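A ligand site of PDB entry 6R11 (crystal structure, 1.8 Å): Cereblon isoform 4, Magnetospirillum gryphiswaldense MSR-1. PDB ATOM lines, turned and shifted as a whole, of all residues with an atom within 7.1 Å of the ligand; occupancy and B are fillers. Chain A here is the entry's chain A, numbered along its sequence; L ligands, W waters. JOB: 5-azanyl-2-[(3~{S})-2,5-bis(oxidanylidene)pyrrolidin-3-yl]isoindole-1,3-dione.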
ATOM      1  N   VAL A  49       5.303  24.408  13.853  1.00  0.00           N
ATOM      2  CA  VAL A  49       5.654  23.663  15.063  1.00  0.00           C
ATOM      3  C   VAL A  49       5.397  24.492  16.315  1.00  0.00           C
ATOM      4  O   VAL A  49       5.259  25.711  16.203  1.00  0.00           O
ATOM      5  CB  VAL A  49       7.157  23.250  15.013  1.00  0.00           C
ATOM      6  CG1 VAL A  49       7.401  22.257  13.847  1.00  0.00           C
ATOM      7  CG2 VAL A  49       8.071  24.439  14.850  1.00  0.00           C
ATOM      8  N   PHE A  50       5.331  23.863  17.487  1.00  0.00           N
ATOM      9  CA  PHE A  50       5.298  24.589  18.735  1.00  0.00           C
ATOM     10  C   PHE A  50       6.255  24.086  19.779  1.00  0.00           C
ATOM     11  O   PHE A  50       6.553  22.880  19.838  1.00  0.00           O
ATOM     12  CB  PHE A  50       3.858  24.669  19.271  1.00  0.00           C
ATOM     13  CG  PHE A  50       3.307  23.452  19.820  1.00  0.00           C
ATOM     14  CD1 PHE A  50       3.570  23.094  21.162  1.00  0.00           C
ATOM     15  CD2 PHE A  50       2.483  22.648  19.076  1.00  0.00           C
ATOM     16  CE1 PHE A  50       3.022  21.938  21.735  1.00  0.00           C
ATOM     17  CE2 PHE A  50       1.920  21.482  19.639  1.00  0.00           C
ATOM     18  CZ  PHE A  50       2.197  21.131  20.973  1.00  0.00           C
ATOM     19  N   ASN A  51       6.774  25.001  20.585  1.00  0.00           N
ATOM     20  CA  ASN A  51       7.680  24.659  21.664  1.00  0.00           C
ATOM     21  C   ASN A  51       6.953  24.353  23.004  1.00  0.00           C
ATOM     22  O   ASN A  51       5.722  24.498  23.103  1.00  0.00           O
ATOM     23  CB  ASN A  51       8.798  25.715  21.756  1.00  0.00           C
ATOM     24  CG  ASN A  51       8.356  27.010  22.342  1.00  0.00           C
ATOM     25  OD1 ASN A  51       7.252  27.146  22.887  1.00  0.00           O
ATOM     26  ND2 ASN A  51       9.259  27.966  22.324  1.00  0.00           N
ATOM     27  N   PRO A  52       7.691  23.916  24.039  1.00  0.00           N
ATOM     28  CA  PRO A  52       6.999  23.568  25.283  1.00  0.00           C
ATOM     29  C   PRO A  52       6.312  24.765  25.946  1.00  0.00           C
ATOM     30  O   PRO A  52       5.420  24.579  26.740  1.00  0.00           O
ATOM     31  CB  PRO A  52       8.088  22.992  26.192  1.00  0.00           C
ATOM     32  CG  PRO A  52       9.135  22.453  25.224  1.00  0.00           C
ATOM     33  CD  PRO A  52       9.062  23.342  23.989  1.00  0.00           C
ATOM     34  N   ALA A  53       6.756  25.984  25.618  1.00  0.00           N
ATOM     35  CA  ALA A  53       6.158  27.203  26.105  1.00  0.00           C
ATOM     36  C   ALA A  53       4.941  27.629  25.241  1.00  0.00           C
ATOM     37  O   ALA A  53       4.407  28.737  25.427  1.00  0.00           O
ATOM     38  CB  ALA A  53       7.203  28.305  26.145  1.00  0.00           C
ATOM     39  N   MET A  55       4.709  28.464  22.104  1.00  0.00           N
ATOM     40  CA  MET A  55       4.932  29.437  21.034  1.00  0.00           C
ATOM     41  C   MET A  55       4.889  28.665  19.721  1.00  0.00           C
ATOM     42  O   MET A  55       5.557  27.611  19.609  1.00  0.00           O
ATOM     43  CB  MET A  55       6.304  30.095  21.177  1.00  0.00           C
ATOM     44  CG  MET A  55       6.529  30.837  22.465  1.00  0.00           C
ATOM     45  SD  MET A  55       8.168  31.551  22.434  1.00  0.00           S
ATOM     46  CE  MET A  55       9.182  30.584  23.565  1.00  0.00           C
ATOM     47  N   PHE A  57       5.723  28.385  15.697  1.00  0.00           N
ATOM     48  CA  PHE A  57       6.715  28.932  14.753  1.00  0.00           C
ATOM     49  C   PHE A  57       6.447  28.333  13.402  1.00  0.00           C
ATOM     50  O   PHE A  57       6.188  27.140  13.263  1.00  0.00           O
ATOM     51  CB  PHE A  57       8.111  28.552  15.160  1.00  0.00           C
ATOM     52  CG  PHE A  57       8.539  29.022  16.524  1.00  0.00           C
ATOM     53  CD1 PHE A  57       9.058  30.256  16.718  1.00  0.00           C
ATOM     54  CD2 PHE A  57       8.470  28.168  17.619  1.00  0.00           C
ATOM     55  CE1 PHE A  57       9.506  30.667  17.982  1.00  0.00           C
ATOM     56  CE2 PHE A  57       8.917  28.569  18.872  1.00  0.00           C
ATOM     57  CZ  PHE A  57       9.435  29.826  19.047  1.00  0.00           C
ATOM     58  N   SER A  75      21.117  19.812  21.999  1.00  0.00           N
ATOM     59  CA  SER A  75      20.173  19.041  22.787  1.00  0.00           C
ATOM     60  C   SER A  75      19.199  18.321  21.870  1.00  0.00           C
ATOM     61  O   SER A  75      18.757  18.884  20.880  1.00  0.00           O
ATOM     62  CB  SER A  75      19.366  19.967  23.692  1.00  0.00           C
ATOM     63  OG  SER A  75      18.426  19.130  24.434  1.00  0.00           O
ATOM     64  N   GLY A  76      18.866  17.081  22.170  1.00  0.00           N
ATOM     65  CA  GLY A  76      17.799  16.332  21.482  1.00  0.00           C
ATOM     66  C   GLY A  76      16.414  16.532  22.050  1.00  0.00           C
ATOM     67  O   GLY A  76      15.445  16.164  21.419  1.00  0.00           O
ATOM     68  N   GLU A  77      16.316  17.138  23.219  1.00  0.00           N
ATOM     69  CA  GLU A  77      14.995  17.356  23.898  1.00  0.00           C
ATOM     70  C   GLU A  77      14.019  18.116  23.016  1.00  0.00           C
ATOM     71  O   GLU A  77      14.327  19.161  22.504  1.00  0.00           O
ATOM     72  CB  GLU A  77      15.165  18.179  25.175  1.00  0.00           C
ATOM     73  CG  GLU A  77      15.999  17.529  26.236  1.00  0.00           C
ATOM     74  CD  GLU A  77      15.643  17.999  27.655  1.00  0.00           C
ATOM     75  OE1 GLU A  77      15.821  17.183  28.603  1.00  0.00           O
ATOM     76  OE2 GLU A  77      15.187  19.156  27.819  1.00  0.00           O
ATOM     77  N   PHE A  78      12.833  17.551  22.854  1.00  0.00           N
ATOM     78  CA  PHE A  78      11.700  18.170  22.135  1.00  0.00           C
ATOM     79  C   PHE A  78      12.009  18.471  20.664  1.00  0.00           C
ATOM     80  O   PHE A  78      11.277  19.221  20.070  1.00  0.00           O
ATOM     81  CB  PHE A  78      11.256  19.484  22.789  1.00  0.00           C
ATOM     82  CG  PHE A  78      11.162  19.447  24.286  1.00  0.00           C
ATOM     83  CD1 PHE A  78      10.181  18.766  24.888  1.00  0.00           C
ATOM     84  CD2 PHE A  78      12.071  20.155  25.069  1.00  0.00           C
ATOM     85  CE1 PHE A  78      10.038  18.752  26.275  1.00  0.00           C
ATOM     86  CE2 PHE A  78      11.984  20.141  26.453  1.00  0.00           C
ATOM     87  CZ  PHE A  78      10.939  19.456  27.053  1.00  0.00           C
ATOM     88  N   SER A  79      13.033  17.860  20.058  1.00  0.00           N
ATOM     89  CA  SER A  79      13.372  18.161  18.724  1.00  0.00           C
ATOM     90  C   SER A  79      12.211  17.904  17.799  1.00  0.00           C
ATOM     91  O   SER A  79      11.624  16.839  17.819  1.00  0.00           O
ATOM     92  CB  SER A  79      14.589  17.347  18.230  1.00  0.00           C
ATOM     93  OG  SER A  79      14.872  17.723  16.893  1.00  0.00           O
ATOM     94  N   TRP A  80      11.937  18.876  16.958  1.00  0.00           N
ATOM     95  CA  TRP A  80      10.901  18.753  15.925  1.00  0.00           C
ATOM     96  C   TRP A  80      11.302  17.878  14.738  1.00  0.00           C
ATOM     97  O   TRP A  80      10.442  17.557  13.899  1.00  0.00           O
ATOM     98  CB  TRP A  80      10.536  20.122  15.396  1.00  0.00           C
ATOM     99  CG  TRP A  80       9.934  21.015  16.425  1.00  0.00           C
ATOM    100  CD1 TRP A  80       8.909  20.737  17.300  1.00  0.00           C
ATOM    101  CD2 TRP A  80      10.317  22.380  16.668  1.00  0.00           C
ATOM    102  NE1 TRP A  80       8.653  21.855  18.088  1.00  0.00           N
ATOM    103  CE2 TRP A  80       9.470  22.879  17.691  1.00  0.00           C
ATOM    104  CE3 TRP A  80      11.262  23.223  16.117  1.00  0.00           C
ATOM    105  CZ2 TRP A  80       9.589  24.161  18.168  1.00  0.00           C
ATOM    106  CZ3 TRP A  80      11.388  24.509  16.599  1.00  0.00           C
ATOM    107  CH2 TRP A  80      10.533  24.971  17.609  1.00  0.00           C
ATOM    108  N   PHE A  81      12.570  17.496  14.654  1.00  0.00           N
ATOM    109  CA  PHE A  81      13.084  16.766  13.511  1.00  0.00           C
ATOM    110  C   PHE A  81      13.778  15.529  14.030  1.00  0.00           C
ATOM    111  O   PHE A  81      14.804  15.616  14.684  1.00  0.00           O
ATOM    112  CB  PHE A  81      14.035  17.653  12.688  1.00  0.00           C
ATOM    113  CG  PHE A  81      13.361  18.858  12.147  1.00  0.00           C
ATOM    114  CD1 PHE A  81      12.594  18.764  11.001  1.00  0.00           C
ATOM    115  CD2 PHE A  81      13.487  20.071  12.775  1.00  0.00           C
ATOM    116  CE1 PHE A  81      12.010  19.914  10.454  1.00  0.00           C
ATOM    117  CE2 PHE A  81      12.855  21.213  12.266  1.00  0.00           C
ATOM    118  CZ  PHE A  81      12.108  21.121  11.090  1.00  0.00           C
ATOM    119  N   TYR A  84      17.698  14.571  15.053  1.00  0.00           N
ATOM    120  CA  TYR A  84      18.520  15.763  15.128  1.00  0.00           C
ATOM    121  C   TYR A  84      18.506  16.386  16.500  1.00  0.00           C
ATOM    122  O   TYR A  84      17.478  16.379  17.198  1.00  0.00           O
ATOM    123  CB  TYR A  84      18.068  16.789  14.125  1.00  0.00           C
ATOM    124  CG  TYR A  84      18.190  16.367  12.692  1.00  0.00           C
ATOM    125  CD1 TYR A  84      19.336  16.583  11.973  1.00  0.00           C
ATOM    126  CD2 TYR A  84      17.102  15.811  12.046  1.00  0.00           C
ATOM    127  CE1 TYR A  84      19.415  16.224  10.630  1.00  0.00           C
ATOM    128  CE2 TYR A  84      17.167  15.443  10.693  1.00  0.00           C
ATOM    129  CZ  TYR A  84      18.363  15.593  10.017  1.00  0.00           C
ATOM    130  OH  TYR A  84      18.437  15.257   8.702  1.00  0.00           O
ATOM    131  N   ASP A  85      19.660  16.944  16.840  1.00  0.00           N
ATOM    132  CA  ASP A  85      19.896  17.688  18.068  1.00  0.00           C
ATOM    133  C   ASP A  85      19.907  19.155  17.628  1.00  0.00           C
ATOM    134  O   ASP A  85      20.294  19.480  16.504  1.00  0.00           O
ATOM    135  CB  ASP A  85      21.234  17.305  18.688  1.00  0.00           C
ATOM    136  CG  ASP A  85      21.341  15.829  18.976  1.00  0.00           C
ATOM    137  OD1 ASP A  85      20.422  15.273  19.615  1.00  0.00           O
ATOM    138  OD2 ASP A  85      22.349  15.212  18.564  1.00  0.00           O
ATOM    139  N   TRP A  86      19.488  20.060  18.511  1.00  0.00           N
ATOM    140  CA  TRP A  86      19.396  21.466  18.141  1.00  0.00           C
ATOM    141  C   TRP A  86      20.254  22.332  19.063  1.00  0.00           C
ATOM    142  O   TRP A  86      20.530  22.005  20.256  1.00  0.00           O
ATOM    143  CB  TRP A  86      17.950  21.981  18.155  1.00  0.00           C
ATOM    144  CG  TRP A  86      17.199  21.740  19.433  1.00  0.00           C
ATOM    145  CD1 TRP A  86      16.373  20.687  19.705  1.00  0.00           C
ATOM    146  CD2 TRP A  86      17.222  22.542  20.629  1.00  0.00           C
ATOM    147  NE1 TRP A  86      15.915  20.770  20.999  1.00  0.00           N
ATOM    148  CE2 TRP A  86      16.462  21.866  21.600  1.00  0.00           C
ATOM    149  CE3 TRP A  86      17.899  23.729  21.009  1.00  0.00           C
ATOM    150  CZ2 TRP A  86      16.284  22.354  22.896  1.00  0.00           C
ATOM    151  CZ3 TRP A  86      17.713  24.235  22.281  1.00  0.00           C
ATOM    152  CH2 TRP A  86      16.873  23.561  23.210  1.00  0.00           C
ATOM    153  N   ILE A  88      20.408  26.723  19.723  1.00  0.00           N
ATOM    154  CA  ILE A  88      19.792  28.015  19.420  1.00  0.00           C
ATOM    155  C   ILE A  88      20.713  28.791  18.499  1.00  0.00           C
ATOM    156  O   ILE A  88      21.956  28.883  18.738  1.00  0.00           O
ATOM    157  CB  ILE A  88      19.544  28.796  20.722  1.00  0.00           C
ATOM    158  CG1 ILE A  88      18.395  28.095  21.476  1.00  0.00           C
ATOM    159  CG2 ILE A  88      19.231  30.263  20.430  1.00  0.00           C
ATOM    160  CD1 ILE A  88      18.373  28.572  22.908  1.00  0.00           C
ATOM    161  N   HIS A  97      16.710  36.105  18.176  1.00  0.00           N
ATOM    162  CA  HIS A  97      16.622  34.666  18.038  1.00  0.00           C
ATOM    163  C   HIS A  97      16.014  34.310  16.703  1.00  0.00           C
ATOM    164  O   HIS A  97      14.824  34.516  16.503  1.00  0.00           O
ATOM    165  CB  HIS A  97      15.826  34.063  19.202  1.00  0.00           C
ATOM    166  CG  HIS A  97      15.608  32.607  19.032  1.00  0.00           C
ATOM    167  ND1 HIS A  97      14.526  31.955  19.580  1.00  0.00           N
ATOM    168  CD2 HIS A  97      16.338  31.654  18.390  1.00  0.00           C
ATOM    169  CE1 HIS A  97      14.601  30.670  19.277  1.00  0.00           C
ATOM    170  NE2 HIS A  97      15.679  30.468  18.548  1.00  0.00           N
ATOM    171  N   TRP A 100      17.200  27.751  14.872  1.00  0.00           N
ATOM    172  CA  TRP A 100      18.001  26.666  15.458  1.00  0.00           C
ATOM    173  C   TRP A 100      18.883  26.052  14.362  1.00  0.00           C
ATOM    174  O   TRP A 100      18.493  26.012  13.205  1.00  0.00           O
ATOM    175  CB  TRP A 100      17.088  25.584  16.053  1.00  0.00           C
ATOM    176  CG  TRP A 100      16.130  26.121  17.091  1.00  0.00           C
ATOM    177  CD1 TRP A 100      16.340  26.162  18.439  1.00  0.00           C
ATOM    178  CD2 TRP A 100      14.864  26.753  16.867  1.00  0.00           C
ATOM    179  NE1 TRP A 100      15.281  26.779  19.052  1.00  0.00           N
ATOM    180  CE2 TRP A 100      14.354  27.128  18.119  1.00  0.00           C
ATOM    181  CE3 TRP A 100      14.093  26.997  15.731  1.00  0.00           C
ATOM    182  CZ2 TRP A 100      13.118  27.749  18.267  1.00  0.00           C
ATOM    183  CZ3 TRP A 100      12.865  27.655  15.874  1.00  0.00           C
ATOM    184  CH2 TRP A 100      12.405  28.057  17.126  1.00  0.00           C
ATOM    185  N   TYR A 102      20.485  22.396  13.477  1.00  0.00           N
ATOM    186  CA  TYR A 102      20.204  20.982  13.772  1.00  0.00           C
ATOM    187  C   TYR A 102      21.409  20.186  13.300  1.00  0.00           C
ATOM    188  O   TYR A 102      21.979  20.489  12.283  1.00  0.00           O
ATOM    189  CB  TYR A 102      18.942  20.518  13.023  1.00  0.00           C
ATOM    190  CG  TYR A 102      17.705  21.088  13.664  1.00  0.00           C
ATOM    191  CD1 TYR A 102      17.136  20.449  14.718  1.00  0.00           C
ATOM    192  CD2 TYR A 102      17.179  22.283  13.230  1.00  0.00           C
ATOM    193  CE1 TYR A 102      15.968  20.998  15.332  1.00  0.00           C
ATOM    194  CE2 TYR A 102      16.060  22.842  13.823  1.00  0.00           C
ATOM    195  CZ  TYR A 102      15.462  22.172  14.888  1.00  0.00           C
ATOM    196  OH  TYR A 102      14.330  22.718  15.513  1.00  0.00           O
HETATM  197  C4  JOB L   1      11.367  22.836  20.365  1.00  0.00           C
HETATM  198  C5  JOB L   1      12.967  23.762  22.763  1.00  0.00           C
HETATM  199  C6  JOB L   1      12.984  24.649  23.951  1.00  0.00           C
HETATM  200  C11 JOB L   1      12.829  26.693  25.786  1.00  0.00           C
HETATM  201  C7  JOB L   1      12.568  25.908  23.557  1.00  0.00           C
HETATM  202  C8  JOB L   1      12.274  25.871  22.109  1.00  0.00           C
HETATM  203  C9  JOB L   1      13.332  24.376  25.251  1.00  0.00           C
HETATM  204  C10 JOB L   1      13.252  25.422  26.180  1.00  0.00           C
HETATM  205  C12 JOB L   1      12.480  26.948  24.465  1.00  0.00           C
HETATM  206  N1  JOB L   1      11.932  21.880  19.571  1.00  0.00           N
HETATM  207  N2  JOB L   1      12.499  24.549  21.714  1.00  0.00           N
HETATM  208  C3  JOB L   1      12.263  24.049  20.369  1.00  0.00           C
HETATM  209  N3  JOB L   1      13.596  25.188  27.511  1.00  0.00           N
HETATM  210  C1  JOB L   1      13.143  22.265  19.046  1.00  0.00           C
HETATM  211  C2  JOB L   1      13.548  23.568  19.677  1.00  0.00           C
HETATM  212  O1  JOB L   1      10.316  22.722  20.970  1.00  0.00           O
HETATM  213  O2  JOB L   1      13.763  21.635  18.200  1.00  0.00           O
HETATM  214  O3  JOB L   1      13.286  22.606  22.665  1.00  0.00           O
HETATM  215  O4  JOB L   1      11.905  26.756  21.370  1.00  0.00           O
HETATM  216  O   HOH W   1      12.719  29.173  21.598  1.00  0.00           O
HETATM  217  O   HOH W   2      15.025  27.158  21.822  1.00  0.00           O
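Water W2 lies within hydrogen-bond range of the indole nitrogen (NE1) of Trp 100 and an oxygen (O4) of the ligand.
The backbone carbonyl oxygen (O) of Phe 78 is in hydrogen-bond range of a nitrogen (N1) of the ligand, at 2.8 Å.
NE1 of Trp 80 sits close to O1 of the ligand (3.4 Å).
O4 of the ligand sits at hydrogen-bond distance from ND2 of Asn 51, at 3.1 Å.
An oxygen (O2) of the ligand lies within hydrogen-bond range of the side-chain hydroxyl of Tyr 102, 3.0 Å away.
The side-chain amide oxygen (OD1) of Asn 51 lies within hydrogen-bond range of the backbone NH (N) of Met 55 (3.0 Å).
The backbone carbonyl oxygen (O) of Tyr 84 lies within hydrogen-bond range of the side-chain hydroxyl (OG) of Ser 79 (2.9 Å).
O of Ser 75 lies within hydrogen-bond range of N of Trp 86, at 2.7 Å.
The side-chain amide oxygen (OD1) of Asn 51 lies within hydrogen-bond range of the backbone NH (N) of Ala 53 (3.0 Å).
The side-chain hydroxyl (OG) of Ser 79 is in hydrogen-bond range of the backbone carbonyl oxygen (O) of Phe 81, 3.1 Å away.
The backbone NH (N) of Glu 77 lies within hydrogen-bond range of the side-chain hydroxyl (OG) of Ser 75, at 3.1 Å.
The indole nitrogen (NE1) of Trp 86 is in hydrogen-bond range of the backbone carbonyl oxygen (O) of Glu 77.
The indole nitrogen of Trp 80 lies within hydrogen-bond range of the backbone carbonyl oxygen of Phe 50, 2.9 Å away.
Residues that only touch the ligand: Trp 86, Pro 52, Trp 100, Ser 79, Glu 77 and Phe 50.
Hydrophobic or aromatic side chains within 4 Å of the ligand: Pro 52, Phe 78, Trp 80, Trp 86, Trp 100 and Tyr 102.
Ten residues have an atom within 4 Å of the ligand: Phe 50, Asn 51, Pro 52, Glu 77, Phe 78, Ser 79, Trp 80, Trp 86, Trp 100 and Tyr 102.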
